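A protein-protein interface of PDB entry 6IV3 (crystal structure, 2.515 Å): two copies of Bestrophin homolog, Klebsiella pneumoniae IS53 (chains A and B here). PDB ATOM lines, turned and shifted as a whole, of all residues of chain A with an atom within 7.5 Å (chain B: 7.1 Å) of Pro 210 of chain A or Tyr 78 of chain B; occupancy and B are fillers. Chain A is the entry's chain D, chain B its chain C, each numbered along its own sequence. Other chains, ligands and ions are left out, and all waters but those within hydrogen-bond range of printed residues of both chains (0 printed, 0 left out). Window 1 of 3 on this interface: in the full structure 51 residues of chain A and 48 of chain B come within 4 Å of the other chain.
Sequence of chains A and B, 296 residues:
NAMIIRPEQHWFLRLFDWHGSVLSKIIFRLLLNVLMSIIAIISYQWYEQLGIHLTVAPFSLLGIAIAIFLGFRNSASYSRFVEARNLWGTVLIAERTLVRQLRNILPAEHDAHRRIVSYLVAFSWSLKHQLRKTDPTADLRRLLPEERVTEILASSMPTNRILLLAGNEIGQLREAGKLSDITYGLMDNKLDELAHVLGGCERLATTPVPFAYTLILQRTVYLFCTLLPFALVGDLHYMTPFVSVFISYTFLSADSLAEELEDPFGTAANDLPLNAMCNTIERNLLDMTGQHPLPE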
ATOM      1  N   PHE A  72      -0.292  22.473 -12.394  1.00  0.00           N
ATOM      2  CA  PHE A  72       0.160  23.404 -11.357  1.00  0.00           C
ATOM      3  C   PHE A  72      -0.800  23.441 -10.163  1.00  0.00           C
ATOM      4  O   PHE A  72      -0.375  23.361  -9.000  1.00  0.00           O
ATOM      5  CB  PHE A  72       0.309  24.802 -11.943  1.00  0.00           C
ATOM      6  CG  PHE A  72       1.620  25.042 -12.630  1.00  0.00           C
ATOM      7  CD1 PHE A  72       2.761  25.317 -11.894  1.00  0.00           C
ATOM      8  CD2 PHE A  72       1.706  25.010 -14.017  1.00  0.00           C
ATOM      9  CE1 PHE A  72       3.960  25.544 -12.518  1.00  0.00           C
ATOM     10  CE2 PHE A  72       2.905  25.232 -14.662  1.00  0.00           C
ATOM     11  CZ  PHE A  72       4.039  25.498 -13.916  1.00  0.00           C
ATOM     12  N   ARG A  73      -2.098  23.583 -10.431  1.00  0.00           N
ATOM     13  CA  ARG A  73      -3.086  23.589  -9.358  1.00  0.00           C
ATOM     14  C   ARG A  73      -2.972  22.338  -8.488  1.00  0.00           C
ATOM     15  O   ARG A  73      -2.817  22.424  -7.264  1.00  0.00           O
ATOM     16  CB  ARG A  73      -4.486  23.709  -9.958  1.00  0.00           C
ATOM     17  CG  ARG A  73      -5.486  24.342  -9.027  1.00  0.00           C
ATOM     18  CD  ARG A  73      -6.133  23.305  -8.150  1.00  0.00           C
ATOM     19  NE  ARG A  73      -6.607  22.166  -8.916  1.00  0.00           N
ATOM     20  CZ  ARG A  73      -7.875  21.970  -9.266  1.00  0.00           C
ATOM     21  NH1 ARG A  73      -8.802  22.855  -8.927  1.00  0.00           N
ATOM     22  NH2 ARG A  73      -8.214  20.890  -9.965  1.00  0.00           N
ATOM     23  N   SER A  75      -0.536  20.410  -8.198  1.00  0.00           N
ATOM     24  CA  SER A  75       0.717  20.572  -7.471  1.00  0.00           C
ATOM     25  C   SER A  75       0.513  21.309  -6.139  1.00  0.00           C
ATOM     26  O   SER A  75       0.976  20.855  -5.082  1.00  0.00           O
ATOM     27  CB  SER A  75       1.696  21.318  -8.363  1.00  0.00           C
ATOM     28  OG  SER A  75       2.970  21.377  -7.801  1.00  0.00           O
ATOM     29  N   ALA A  76      -0.181  22.453  -6.165  1.00  0.00           N
ATOM     30  CA  ALA A  76      -0.378  23.205  -4.927  1.00  0.00           C
ATOM     31  C   ALA A  76      -1.211  22.413  -3.925  1.00  0.00           C
ATOM     32  O   ALA A  76      -0.859  22.330  -2.732  1.00  0.00           O
ATOM     33  CB  ALA A  76      -1.028  24.561  -5.222  1.00  0.00           C
ATOM     34  N   SER A  77      -2.315  21.817  -4.392  1.00  0.00           N
ATOM     35  CA  SER A  77      -3.128  20.981  -3.514  1.00  0.00           C
ATOM     36  C   SER A  77      -2.275  19.902  -2.856  1.00  0.00           C
ATOM     37  O   SER A  77      -2.317  19.700  -1.633  1.00  0.00           O
ATOM     38  CB  SER A  77      -4.274  20.343  -4.308  1.00  0.00           C
ATOM     39  OG  SER A  77      -5.066  21.301  -4.975  1.00  0.00           O
ATOM     40  N   SER A  79       0.953  19.776  -2.285  1.00  0.00           N
ATOM     41  CA  SER A  79       1.922  20.230  -1.296  1.00  0.00           C
ATOM     42  C   SER A  79       1.230  20.623   0.005  1.00  0.00           C
ATOM     43  O   SER A  79       1.817  20.486   1.089  1.00  0.00           O
ATOM     44  CB  SER A  79       2.753  21.386  -1.857  1.00  0.00           C
ATOM     45  OG  SER A  79       2.053  22.607  -1.729  1.00  0.00           O
ATOM     46  N   ARG A  80      -0.029  21.068  -0.115  1.00  0.00           N
ATOM     47  CA  ARG A  80      -0.878  21.421   1.058  1.00  0.00           C
ATOM     48  C   ARG A  80      -1.143  20.152   1.883  1.00  0.00           C
ATOM     49  O   ARG A  80      -1.035  20.223   3.123  1.00  0.00           O
ATOM     50  CB  ARG A  80      -2.191  22.062   0.595  1.00  0.00           C
ATOM     51  CG  ARG A  80      -3.040  22.625   1.725  1.00  0.00           C
ATOM     52  CD  ARG A  80      -4.222  23.428   1.216  1.00  0.00           C
ATOM     53  NE  ARG A  80      -5.464  23.070   1.884  1.00  0.00           N
ATOM     54  CZ  ARG A  80      -5.903  23.630   3.006  1.00  0.00           C
ATOM     55  NH1 ARG A  80      -5.197  24.582   3.591  1.00  0.00           N
ATOM     56  NH2 ARG A  80      -7.047  23.237   3.539  1.00  0.00           N
ATOM     57  N   THR A 207      -6.612  28.181   5.793  1.00  0.00           N
ATOM     58  CA  THR A 207      -5.969  28.790   4.626  1.00  0.00           C
ATOM     59  C   THR A 207      -5.945  27.809   3.467  1.00  0.00           C
ATOM     60  O   THR A 207      -5.026  26.974   3.375  1.00  0.00           O
ATOM     61  CB  THR A 207      -4.546  29.259   4.931  1.00  0.00           C
ATOM     62  OG1 THR A 207      -4.539  30.125   6.087  1.00  0.00           O
ATOM     63  CG2 THR A 207      -3.981  29.989   3.699  1.00  0.00           C
ATOM     64  N   PRO A 208      -6.906  27.879   2.551  1.00  0.00           N
ATOM     65  CA  PRO A 208      -6.902  26.982   1.392  1.00  0.00           C
ATOM     66  C   PRO A 208      -6.158  27.587   0.207  1.00  0.00           C
ATOM     67  O   PRO A 208      -5.973  28.806   0.100  1.00  0.00           O
ATOM     68  CB  PRO A 208      -8.399  26.818   1.081  1.00  0.00           C
ATOM     69  CG  PRO A 208      -8.978  28.161   1.452  1.00  0.00           C
ATOM     70  CD  PRO A 208      -8.144  28.680   2.629  1.00  0.00           C
ATOM     71  N   VAL A 209      -5.725  26.705  -0.692  1.00  0.00           N
ATOM     72  CA  VAL A 209      -5.249  27.216  -1.980  1.00  0.00           C
ATOM     73  C   VAL A 209      -6.380  28.008  -2.626  1.00  0.00           C
ATOM     74  O   VAL A 209      -7.510  27.487  -2.735  1.00  0.00           O
ATOM     75  CB  VAL A 209      -4.768  26.063  -2.885  1.00  0.00           C
ATOM     76  CG1 VAL A 209      -5.789  24.931  -2.923  1.00  0.00           C
ATOM     77  CG2 VAL A 209      -4.475  26.573  -4.310  1.00  0.00           C
ATOM     78  N   PRO A 210      -6.147  29.282  -3.019  1.00  0.00           N
ATOM     79  CA  PRO A 210      -7.246  30.163  -3.442  1.00  0.00           C
ATOM     80  C   PRO A 210      -8.234  29.463  -4.356  1.00  0.00           C
ATOM     81  O   PRO A 210      -7.874  28.967  -5.431  1.00  0.00           O
ATOM     82  CB  PRO A 210      -6.519  31.297  -4.171  1.00  0.00           C
ATOM     83  CG  PRO A 210      -5.178  31.352  -3.511  1.00  0.00           C
ATOM     84  CD  PRO A 210      -4.832  29.928  -3.177  1.00  0.00           C
ATOM     85  N   PHE A 211      -9.482  29.369  -3.892  1.00  0.00           N
ATOM     86  CA  PHE A 211     -10.516  28.645  -4.623  1.00  0.00           C
ATOM     87  C   PHE A 211     -10.952  29.341  -5.901  1.00  0.00           C
ATOM     88  O   PHE A 211     -11.741  28.767  -6.659  1.00  0.00           O
ATOM     89  CB  PHE A 211     -11.749  28.417  -3.745  1.00  0.00           C
ATOM     90  CG  PHE A 211     -11.514  27.474  -2.603  1.00  0.00           C
ATOM     91  CD1 PHE A 211     -10.495  26.527  -2.693  1.00  0.00           C
ATOM     92  CD2 PHE A 211     -12.316  27.489  -1.470  1.00  0.00           C
ATOM     93  CE1 PHE A 211     -10.270  25.644  -1.638  1.00  0.00           C
ATOM     94  CE2 PHE A 211     -12.096  26.618  -0.424  1.00  0.00           C
ATOM     95  CZ  PHE A 211     -11.082  25.689  -0.510  1.00  0.00           C
ATOM     96  N   ALA A 212     -10.493  30.569  -6.147  1.00  0.00           N
ATOM     97  CA  ALA A 212     -10.644  31.138  -7.482  1.00  0.00           C
ATOM     98  C   ALA A 212     -10.056  30.204  -8.542  1.00  0.00           C
ATOM     99  O   ALA A 212     -10.688  29.929  -9.572  1.00  0.00           O
ATOM    100  CB  ALA A 212      -9.975  32.510  -7.541  1.00  0.00           C
ATOM    101  N   TYR A 213      -8.830  29.732  -8.305  1.00  0.00           N
ATOM    102  CA  TYR A 213      -8.214  28.662  -9.077  1.00  0.00           C
ATOM    103  C   TYR A 213      -9.229  27.571  -9.331  1.00  0.00           C
ATOM    104  O   TYR A 213      -9.599  27.297 -10.475  1.00  0.00           O
ATOM    105  CB  TYR A 213      -7.036  28.024  -8.332  1.00  0.00           C
ATOM    106  CG  TYR A 213      -5.797  28.863  -8.228  1.00  0.00           C
ATOM    107  CD1 TYR A 213      -5.410  29.706  -9.264  1.00  0.00           C
ATOM    108  CD2 TYR A 213      -5.000  28.803  -7.092  1.00  0.00           C
ATOM    109  CE1 TYR A 213      -4.266  30.473  -9.165  1.00  0.00           C
ATOM    110  CE2 TYR A 213      -3.857  29.558  -6.981  1.00  0.00           C
ATOM    111  CZ  TYR A 213      -3.489  30.391  -8.021  1.00  0.00           C
ATOM    112  OH  TYR A 213      -2.344  31.150  -7.914  1.00  0.00           O
ATOM    113  N   THR A 214      -9.686  26.958  -8.241  1.00  0.00           N
ATOM    114  CA  THR A 214     -10.457  25.728  -8.340  1.00  0.00           C
ATOM    115  C   THR A 214     -11.782  25.954  -9.048  1.00  0.00           C
ATOM    116  O   THR A 214     -12.251  25.093  -9.800  1.00  0.00           O
ATOM    117  CB  THR A 214     -10.669  25.163  -6.938  1.00  0.00           C
ATOM    118  OG1 THR A 214      -9.454  24.542  -6.489  1.00  0.00           O
ATOM    119  CG2 THR A 214     -11.818  24.172  -6.911  1.00  0.00           C
ATOM    120  N   LEU A 215     -12.382  27.121  -8.838  1.00  0.00           N
ATOM    121  CA  LEU A 215     -13.713  27.402  -9.348  1.00  0.00           C
ATOM    122  C   LEU A 215     -13.669  27.707 -10.838  1.00  0.00           C
ATOM    123  O   LEU A 215     -14.314  27.020 -11.638  1.00  0.00           O
ATOM    124  CB  LEU A 215     -14.331  28.564  -8.570  1.00  0.00           C
ATOM    125  CG  LEU A 215     -15.610  29.139  -9.180  1.00  0.00           C
ATOM    126  CD1 LEU A 215     -16.820  28.239  -8.892  1.00  0.00           C
ATOM    127  CD2 LEU A 215     -15.855  30.578  -8.733  1.00  0.00           C
ATOM    128  N   GLU A 262      -7.829  18.902  -0.657  1.00  0.00           N
ATOM    129  CA  GLU A 262      -7.993  20.284  -0.208  1.00  0.00           C
ATOM    130  C   GLU A 262      -8.068  20.382   1.311  1.00  0.00           C
ATOM    131  O   GLU A 262      -7.492  21.307   1.900  1.00  0.00           O
ATOM    132  CB  GLU A 262      -9.231  20.913  -0.854  1.00  0.00           C
ATOM    133  CG  GLU A 262      -9.097  21.111  -2.361  1.00  0.00           C
ATOM    134  CD  GLU A 262      -8.097  22.193  -2.731  1.00  0.00           C
ATOM    135  OE1 GLU A 262      -8.533  23.312  -3.106  1.00  0.00           O
ATOM    136  OE2 GLU A 262      -6.876  21.916  -2.636  1.00  0.00           O
ATOM    137  N   ARG B  73       4.560  31.756 -13.852  1.00  0.00           N
ATOM    138  CA  ARG B  73       4.339  33.017 -13.158  1.00  0.00           C
ATOM    139  C   ARG B  73       3.303  32.864 -12.045  1.00  0.00           C
ATOM    140  O   ARG B  73       3.505  33.344 -10.917  1.00  0.00           O
ATOM    141  CB  ARG B  73       3.920  34.091 -14.151  1.00  0.00           C
ATOM    142  CG  ARG B  73       4.362  35.484 -13.730  1.00  0.00           C
ATOM    143  CD  ARG B  73       3.309  36.121 -12.869  1.00  0.00           C
ATOM    144  NE  ARG B  73       1.987  35.807 -13.388  1.00  0.00           N
ATOM    145  CZ  ARG B  73       1.313  36.585 -14.229  1.00  0.00           C
ATOM    146  NH1 ARG B  73       1.839  37.730 -14.643  1.00  0.00           N
ATOM    147  NH2 ARG B  73       0.105  36.214 -14.643  1.00  0.00           N
ATOM    148  N   ASN B  74       2.183  32.194 -12.348  1.00  0.00           N
ATOM    149  CA  ASN B  74       1.178  31.931 -11.323  1.00  0.00           C
ATOM    150  C   ASN B  74       1.800  31.211 -10.132  1.00  0.00           C
ATOM    151  O   ASN B  74       1.510  31.536  -8.977  1.00  0.00           O
ATOM    152  CB  ASN B  74       0.016  31.114 -11.906  1.00  0.00           C
ATOM    153  CG  ASN B  74      -1.175  31.981 -12.324  1.00  0.00           C
ATOM    154  OD1 ASN B  74      -2.117  32.156 -11.553  1.00  0.00           O
ATOM    155  ND2 ASN B  74      -1.148  32.503 -13.547  1.00  0.00           N
ATOM    156  N   SER B  75       2.673  30.238 -10.401  1.00  0.00           N
ATOM    157  CA  SER B  75       3.391  29.547  -9.339  1.00  0.00           C
ATOM    158  C   SER B  75       4.168  30.525  -8.457  1.00  0.00           C
ATOM    159  O   SER B  75       4.189  30.390  -7.223  1.00  0.00           O
ATOM    160  CB  SER B  75       4.326  28.530  -9.972  1.00  0.00           C
ATOM    161  OG  SER B  75       5.287  28.065  -9.056  1.00  0.00           O
ATOM    162  N   ALA B  76       4.814  31.520  -9.072  1.00  0.00           N
ATOM    163  CA  ALA B  76       5.494  32.540  -8.281  1.00  0.00           C
ATOM    164  C   ALA B  76       4.515  33.287  -7.374  1.00  0.00           C
ATOM    165  O   ALA B  76       4.729  33.382  -6.156  1.00  0.00           O
ATOM    166  CB  ALA B  76       6.232  33.514  -9.195  1.00  0.00           C
ATOM    167  N   SER B  77       3.429  33.815  -7.950  1.00  0.00           N
ATOM    168  CA  SER B  77       2.450  34.587  -7.181  1.00  0.00           C
ATOM    169  C   SER B  77       1.907  33.781  -6.008  1.00  0.00           C
ATOM    170  O   SER B  77       1.990  34.194  -4.842  1.00  0.00           O
ATOM    171  CB  SER B  77       1.302  35.016  -8.091  1.00  0.00           C
ATOM    172  OG  SER B  77       1.795  35.538  -9.313  1.00  0.00           O
ATOM    173  N   TYR B  78       1.332  32.623  -6.314  1.00  0.00           N
ATOM    174  CA  TYR B  78       0.859  31.705  -5.292  1.00  0.00           C
ATOM    175  C   TYR B  78       1.867  31.522  -4.167  1.00  0.00           C
ATOM    176  O   TYR B  78       1.509  31.578  -2.985  1.00  0.00           O
ATOM    177  CB  TYR B  78       0.556  30.356  -5.919  1.00  0.00           C
ATOM    178  CG  TYR B  78       0.065  29.356  -4.909  1.00  0.00           C
ATOM    179  CD1 TYR B  78      -1.193  29.485  -4.333  1.00  0.00           C
ATOM    180  CD2 TYR B  78       0.868  28.295  -4.508  1.00  0.00           C
ATOM    181  CE1 TYR B  78      -1.649  28.575  -3.417  1.00  0.00           C
ATOM    182  CE2 TYR B  78       0.420  27.382  -3.594  1.00  0.00           C
ATOM    183  CZ  TYR B  78      -0.847  27.527  -3.055  1.00  0.00           C
ATOM    184  OH  TYR B  78      -1.301  26.611  -2.143  1.00  0.00           O
ATOM    185  N   SER B  79       3.137  31.274  -4.505  1.00  0.00           N
ATOM    186  CA  SER B  79       4.058  31.006  -3.410  1.00  0.00           C
ATOM    187  C   SER B  79       4.328  32.278  -2.601  1.00  0.00           C
ATOM    188  O   SER B  79       4.545  32.199  -1.385  1.00  0.00           O
ATOM    189  CB  SER B  79       5.332  30.348  -3.937  1.00  0.00           C
ATOM    190  OG  SER B  79       6.201  31.315  -4.444  1.00  0.00           O
ATOM    191  N   ARG B  80       4.224  33.454  -3.225  1.00  0.00           N
ATOM    192  CA  ARG B  80       4.298  34.704  -2.469  1.00  0.00           C
ATOM    193  C   ARG B  80       3.150  34.809  -1.459  1.00  0.00           C
ATOM    194  O   ARG B  80       3.339  35.247  -0.307  1.00  0.00           O
ATOM    195  CB  ARG B  80       4.276  35.890  -3.435  1.00  0.00           C
ATOM    196  CG  ARG B  80       5.112  37.058  -3.009  1.00  0.00           C
ATOM    197  CD  ARG B  80       5.414  38.051  -4.144  1.00  0.00           C
ATOM    198  NE  ARG B  80       5.524  39.417  -3.618  1.00  0.00           N
ATOM    199  CZ  ARG B  80       4.487  40.226  -3.416  1.00  0.00           C
ATOM    200  NH1 ARG B  80       3.255  39.812  -3.698  1.00  0.00           N
ATOM    201  NH2 ARG B  80       4.677  41.443  -2.924  1.00  0.00           N
ATOM    202  N   PHE B  81       1.950  34.388  -1.867  1.00  0.00           N
ATOM    203  CA  PHE B  81       0.789  34.476  -0.989  1.00  0.00           C
ATOM    204  C   PHE B  81       0.882  33.461   0.153  1.00  0.00           C
ATOM    205  O   PHE B  81       0.507  33.745   1.303  1.00  0.00           O
ATOM    206  CB  PHE B  81      -0.466  34.264  -1.827  1.00  0.00           C
ATOM    207  CG  PHE B  81      -1.662  33.808  -1.042  1.00  0.00           C
ATOM    208  CD1 PHE B  81      -1.882  32.450  -0.750  1.00  0.00           C
ATOM    209  CD2 PHE B  81      -2.587  34.747  -0.611  1.00  0.00           C
ATOM    210  CE1 PHE B  81      -2.997  32.048  -0.024  1.00  0.00           C
ATOM    211  CE2 PHE B  81      -3.688  34.360   0.101  1.00  0.00           C
ATOM    212  CZ  PHE B  81      -3.898  33.001   0.406  1.00  0.00           C
ATOM    213  N   VAL B  82       1.400  32.277  -0.144  1.00  0.00           N
ATOM    214  CA  VAL B  82       1.601  31.279   0.892  1.00  0.00           C
ATOM    215  C   VAL B  82       2.625  31.772   1.905  1.00  0.00           C
ATOM    216  O   VAL B  82       2.477  31.547   3.111  1.00  0.00           O
ATOM    217  CB  VAL B  82       2.018  29.945   0.248  1.00  0.00           C
ATOM    218  CG1 VAL B  82       2.458  28.949   1.307  1.00  0.00           C
ATOM    219  CG2 VAL B  82       0.876  29.386  -0.601  1.00  0.00           C
ATOM    220  N   GLU B  83       3.668  32.468   1.443  1.00  0.00           N
ATOM    221  CA  GLU B  83       4.652  32.955   2.396  1.00  0.00           C
ATOM    222  C   GLU B  83       4.048  34.013   3.309  1.00  0.00           C
ATOM    223  O   GLU B  83       4.307  34.011   4.516  1.00  0.00           O
ATOM    224  CB  GLU B  83       5.889  33.506   1.689  1.00  0.00           C
ATOM    225  CG  GLU B  83       7.009  33.783   2.697  1.00  0.00           C
ATOM    226  CD  GLU B  83       8.320  34.282   2.098  1.00  0.00           C
ATOM    227  OE1 GLU B  83       8.418  34.434   0.863  1.00  0.00           O
ATOM    228  OE2 GLU B  83       9.264  34.523   2.879  1.00  0.00           O
ATOM    229  N   ALA B  84       3.256  34.934   2.751  1.00  0.00           N
ATOM    230  CA  ALA B  84       2.649  35.967   3.584  1.00  0.00           C
ATOM    231  C   ALA B  84       1.792  35.345   4.685  1.00  0.00           C
ATOM    232  O   ALA B  84       1.913  35.702   5.876  1.00  0.00           O
ATOM    233  CB  ALA B  84       1.825  36.913   2.713  1.00  0.00           C
ATOM    234  N   VAL B 209       6.576  40.222  -7.512  1.00  0.00           N
ATOM    235  CA  VAL B 209       7.006  39.473  -8.702  1.00  0.00           C
ATOM    236  C   VAL B 209       7.436  40.475  -9.770  1.00  0.00           C
ATOM    237  O   VAL B 209       6.653  41.395 -10.092  1.00  0.00           O
ATOM    238  CB  VAL B 209       5.871  38.562  -9.223  1.00  0.00           C
ATOM    239  CG1 VAL B 209       6.396  37.593 -10.274  1.00  0.00           C
ATOM    240  CG2 VAL B 209       5.215  37.786  -8.092  1.00  0.00           C
ATOM    241  N   LEU B 257      -5.483  36.246 -12.411  1.00  0.00           N
ATOM    242  CA  LEU B 257      -5.440  35.631 -11.081  1.00  0.00           C
ATOM    243  C   LEU B 257      -4.101  35.880 -10.395  1.00  0.00           C
ATOM    244  O   LEU B 257      -4.042  36.106  -9.176  1.00  0.00           O
ATOM    245  CB  LEU B 257      -5.717  34.131 -11.182  1.00  0.00           C
ATOM    246  CG  LEU B 257      -6.670  33.506 -10.159  1.00  0.00           C
ATOM    247  CD1 LEU B 257      -7.801  34.478  -9.831  1.00  0.00           C
ATOM    248  CD2 LEU B 257      -7.237  32.181 -10.677  1.00  0.00           C
ATOM    249  N   ALA B 258      -3.018  35.870 -11.166  1.00  0.00           N
ATOM    250  CA  ALA B 258      -1.706  36.104 -10.581  1.00  0.00           C
ATOM    251  C   ALA B 258      -1.582  37.524 -10.060  1.00  0.00           C
ATOM    252  O   ALA B 258      -1.029  37.741  -8.975  1.00  0.00           O
ATOM    253  CB  ALA B 258      -0.617  35.812 -11.603  1.00  0.00           C
ATOM    254  N   GLU B 260      -4.123  39.160  -9.122  1.00  0.00           N
ATOM    255  CA  GLU B 260      -5.095  39.203  -8.045  1.00  0.00           C
ATOM    256  C   GLU B 260      -4.518  38.626  -6.763  1.00  0.00           C
ATOM    257  O   GLU B 260      -5.069  38.862  -5.687  1.00  0.00           O
ATOM    258  CB  GLU B 260      -6.362  38.470  -8.500  1.00  0.00           C
ATOM    259  CG  GLU B 260      -7.114  37.673  -7.479  1.00  0.00           C
ATOM    260  CD  GLU B 260      -8.530  37.416  -7.946  1.00  0.00           C
ATOM    261  OE1 GLU B 260      -8.788  37.628  -9.157  1.00  0.00           O
ATOM    262  OE2 GLU B 260      -9.384  37.040  -7.109  1.00  0.00           O
ATOM    263  N   LEU B 261      -3.405  37.896  -6.856  1.00  0.00           N
ATOM    264  CA  LEU B 261      -2.564  37.596  -5.707  1.00  0.00           C
ATOM    265  C   LEU B 261      -1.349  38.513  -5.638  1.00  0.00           C
ATOM    266  O   LEU B 261      -0.293  38.098  -5.144  1.00  0.00           O
ATOM    267  CB  LEU B 261      -2.117  36.134  -5.730  1.00  0.00           C
ATOM    268  CG  LEU B 261      -3.183  35.054  -5.893  1.00  0.00           C
ATOM    269  CD1 LEU B 261      -2.674  33.726  -5.371  1.00  0.00           C
ATOM    270  CD2 LEU B 261      -4.458  35.451  -5.165  1.00  0.00           C
ATOM    271  N   ASN B 270      -9.519  38.505  -1.944  1.00  0.00           N
ATOM    272  CA  ASN B 270      -8.480  37.482  -1.978  1.00  0.00           C
ATOM    273  C   ASN B 270      -7.341  37.758  -1.002  1.00  0.00           C
ATOM    274  O   ASN B 270      -6.585  36.834  -0.680  1.00  0.00           O
ATOM    275  CB  ASN B 270      -7.924  37.341  -3.401  1.00  0.00           C
ATOM    276  CG  ASN B 270      -8.696  36.317  -4.235  1.00  0.00           C
ATOM    277  OD1 ASN B 270      -9.912  36.436  -4.410  1.00  0.00           O
ATOM    278  ND2 ASN B 270      -7.989  35.316  -4.761  1.00  0.00           N
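OG of Ser 79 of chain A lies within hydrogen-bond range of O of Ala 76 of chain A, 3.1 Å away.
Among the printed residues, merely in contact across the chains: Tyr 213 of chain A with Leu 257 of chain B (3.4 Å), Pro 210 of chain A with Tyr 78 of chain B (3.5 Å), Ala 76 of chain A with Tyr 78 of chain B (3.6 Å), Val 209 of chain A with Tyr 78 of chain B (3.6 Å), Tyr 213 of chain A with Tyr 78 of chain B (3.6 Å), Tyr 213 of chain A with Asn 74 of chain B (3.6 Å), Tyr 213 of chain A with Leu 261 of chain B (3.6 Å), Ala 212 of chain A with Leu 257 of chain B (3.7 Å), Pro 210 of chain A with Leu 261 of chain B (3.9 Å) and Phe 72 of chain A with Ser 75 of chain B (3.9 Å).
Of the printed residues of chain B, Pro 210 of chain A touches Tyr 78 and Leu 261.
Printed residues of chain A within 4 Å of Leu 257 of chain B: Ala 212 (3.7 Å) and Tyr 213 (3.4 Å).
Of the printed residues of chain B, Ala 212 of chain A touches Leu 257 (3.7 Å).
Of the printed residues of chain B, Tyr 213 of chain A touches Asn 74 (3.6 Å), Tyr 78 (3.6 Å), Leu 257 (3.4 Å) and Leu 261 (3.6 Å).
Of the printed residues of chain A, Ser 75 of chain B touches Phe 72 (3.9 Å).
Of the printed residues of chain B, Val 209 of chain A touches Tyr 78.
Phe 211 of chain A touches none of the printed residues of chain B.
The nearest residue of chain A that does not touch Tyr 78 of chain B is Ser 79 of chain A (5.2 Å).
Of the 17 printed residues of chain A, 6 touch a printed residue of chain B.
Hydrophobic or aromatic side chains of chain A within 4 Å of the printed part of chain B: Phe 72, Ala 76, Val 209, Pro 210, Ala 212 and Tyr 213.
Of the 18 printed residues of chain B, 5 touch a printed residue of chain A.
Printed residues of chain B that touch a printed residue of chain A: Asn 74, Ser 75, Tyr 78, Leu 257 and Leu 261.
Among the printed residues, no Asp or Glu carboxylate lies within 4 Å of a Lys or Arg side-chain nitrogen of the other chain.
Positions printed for both chains: 73, 75, 76, 77, 79, 80 and 209.
Of the 10 pairs that touch across the chains among the printed residues, none has its exchanged pair printed and touching as well.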
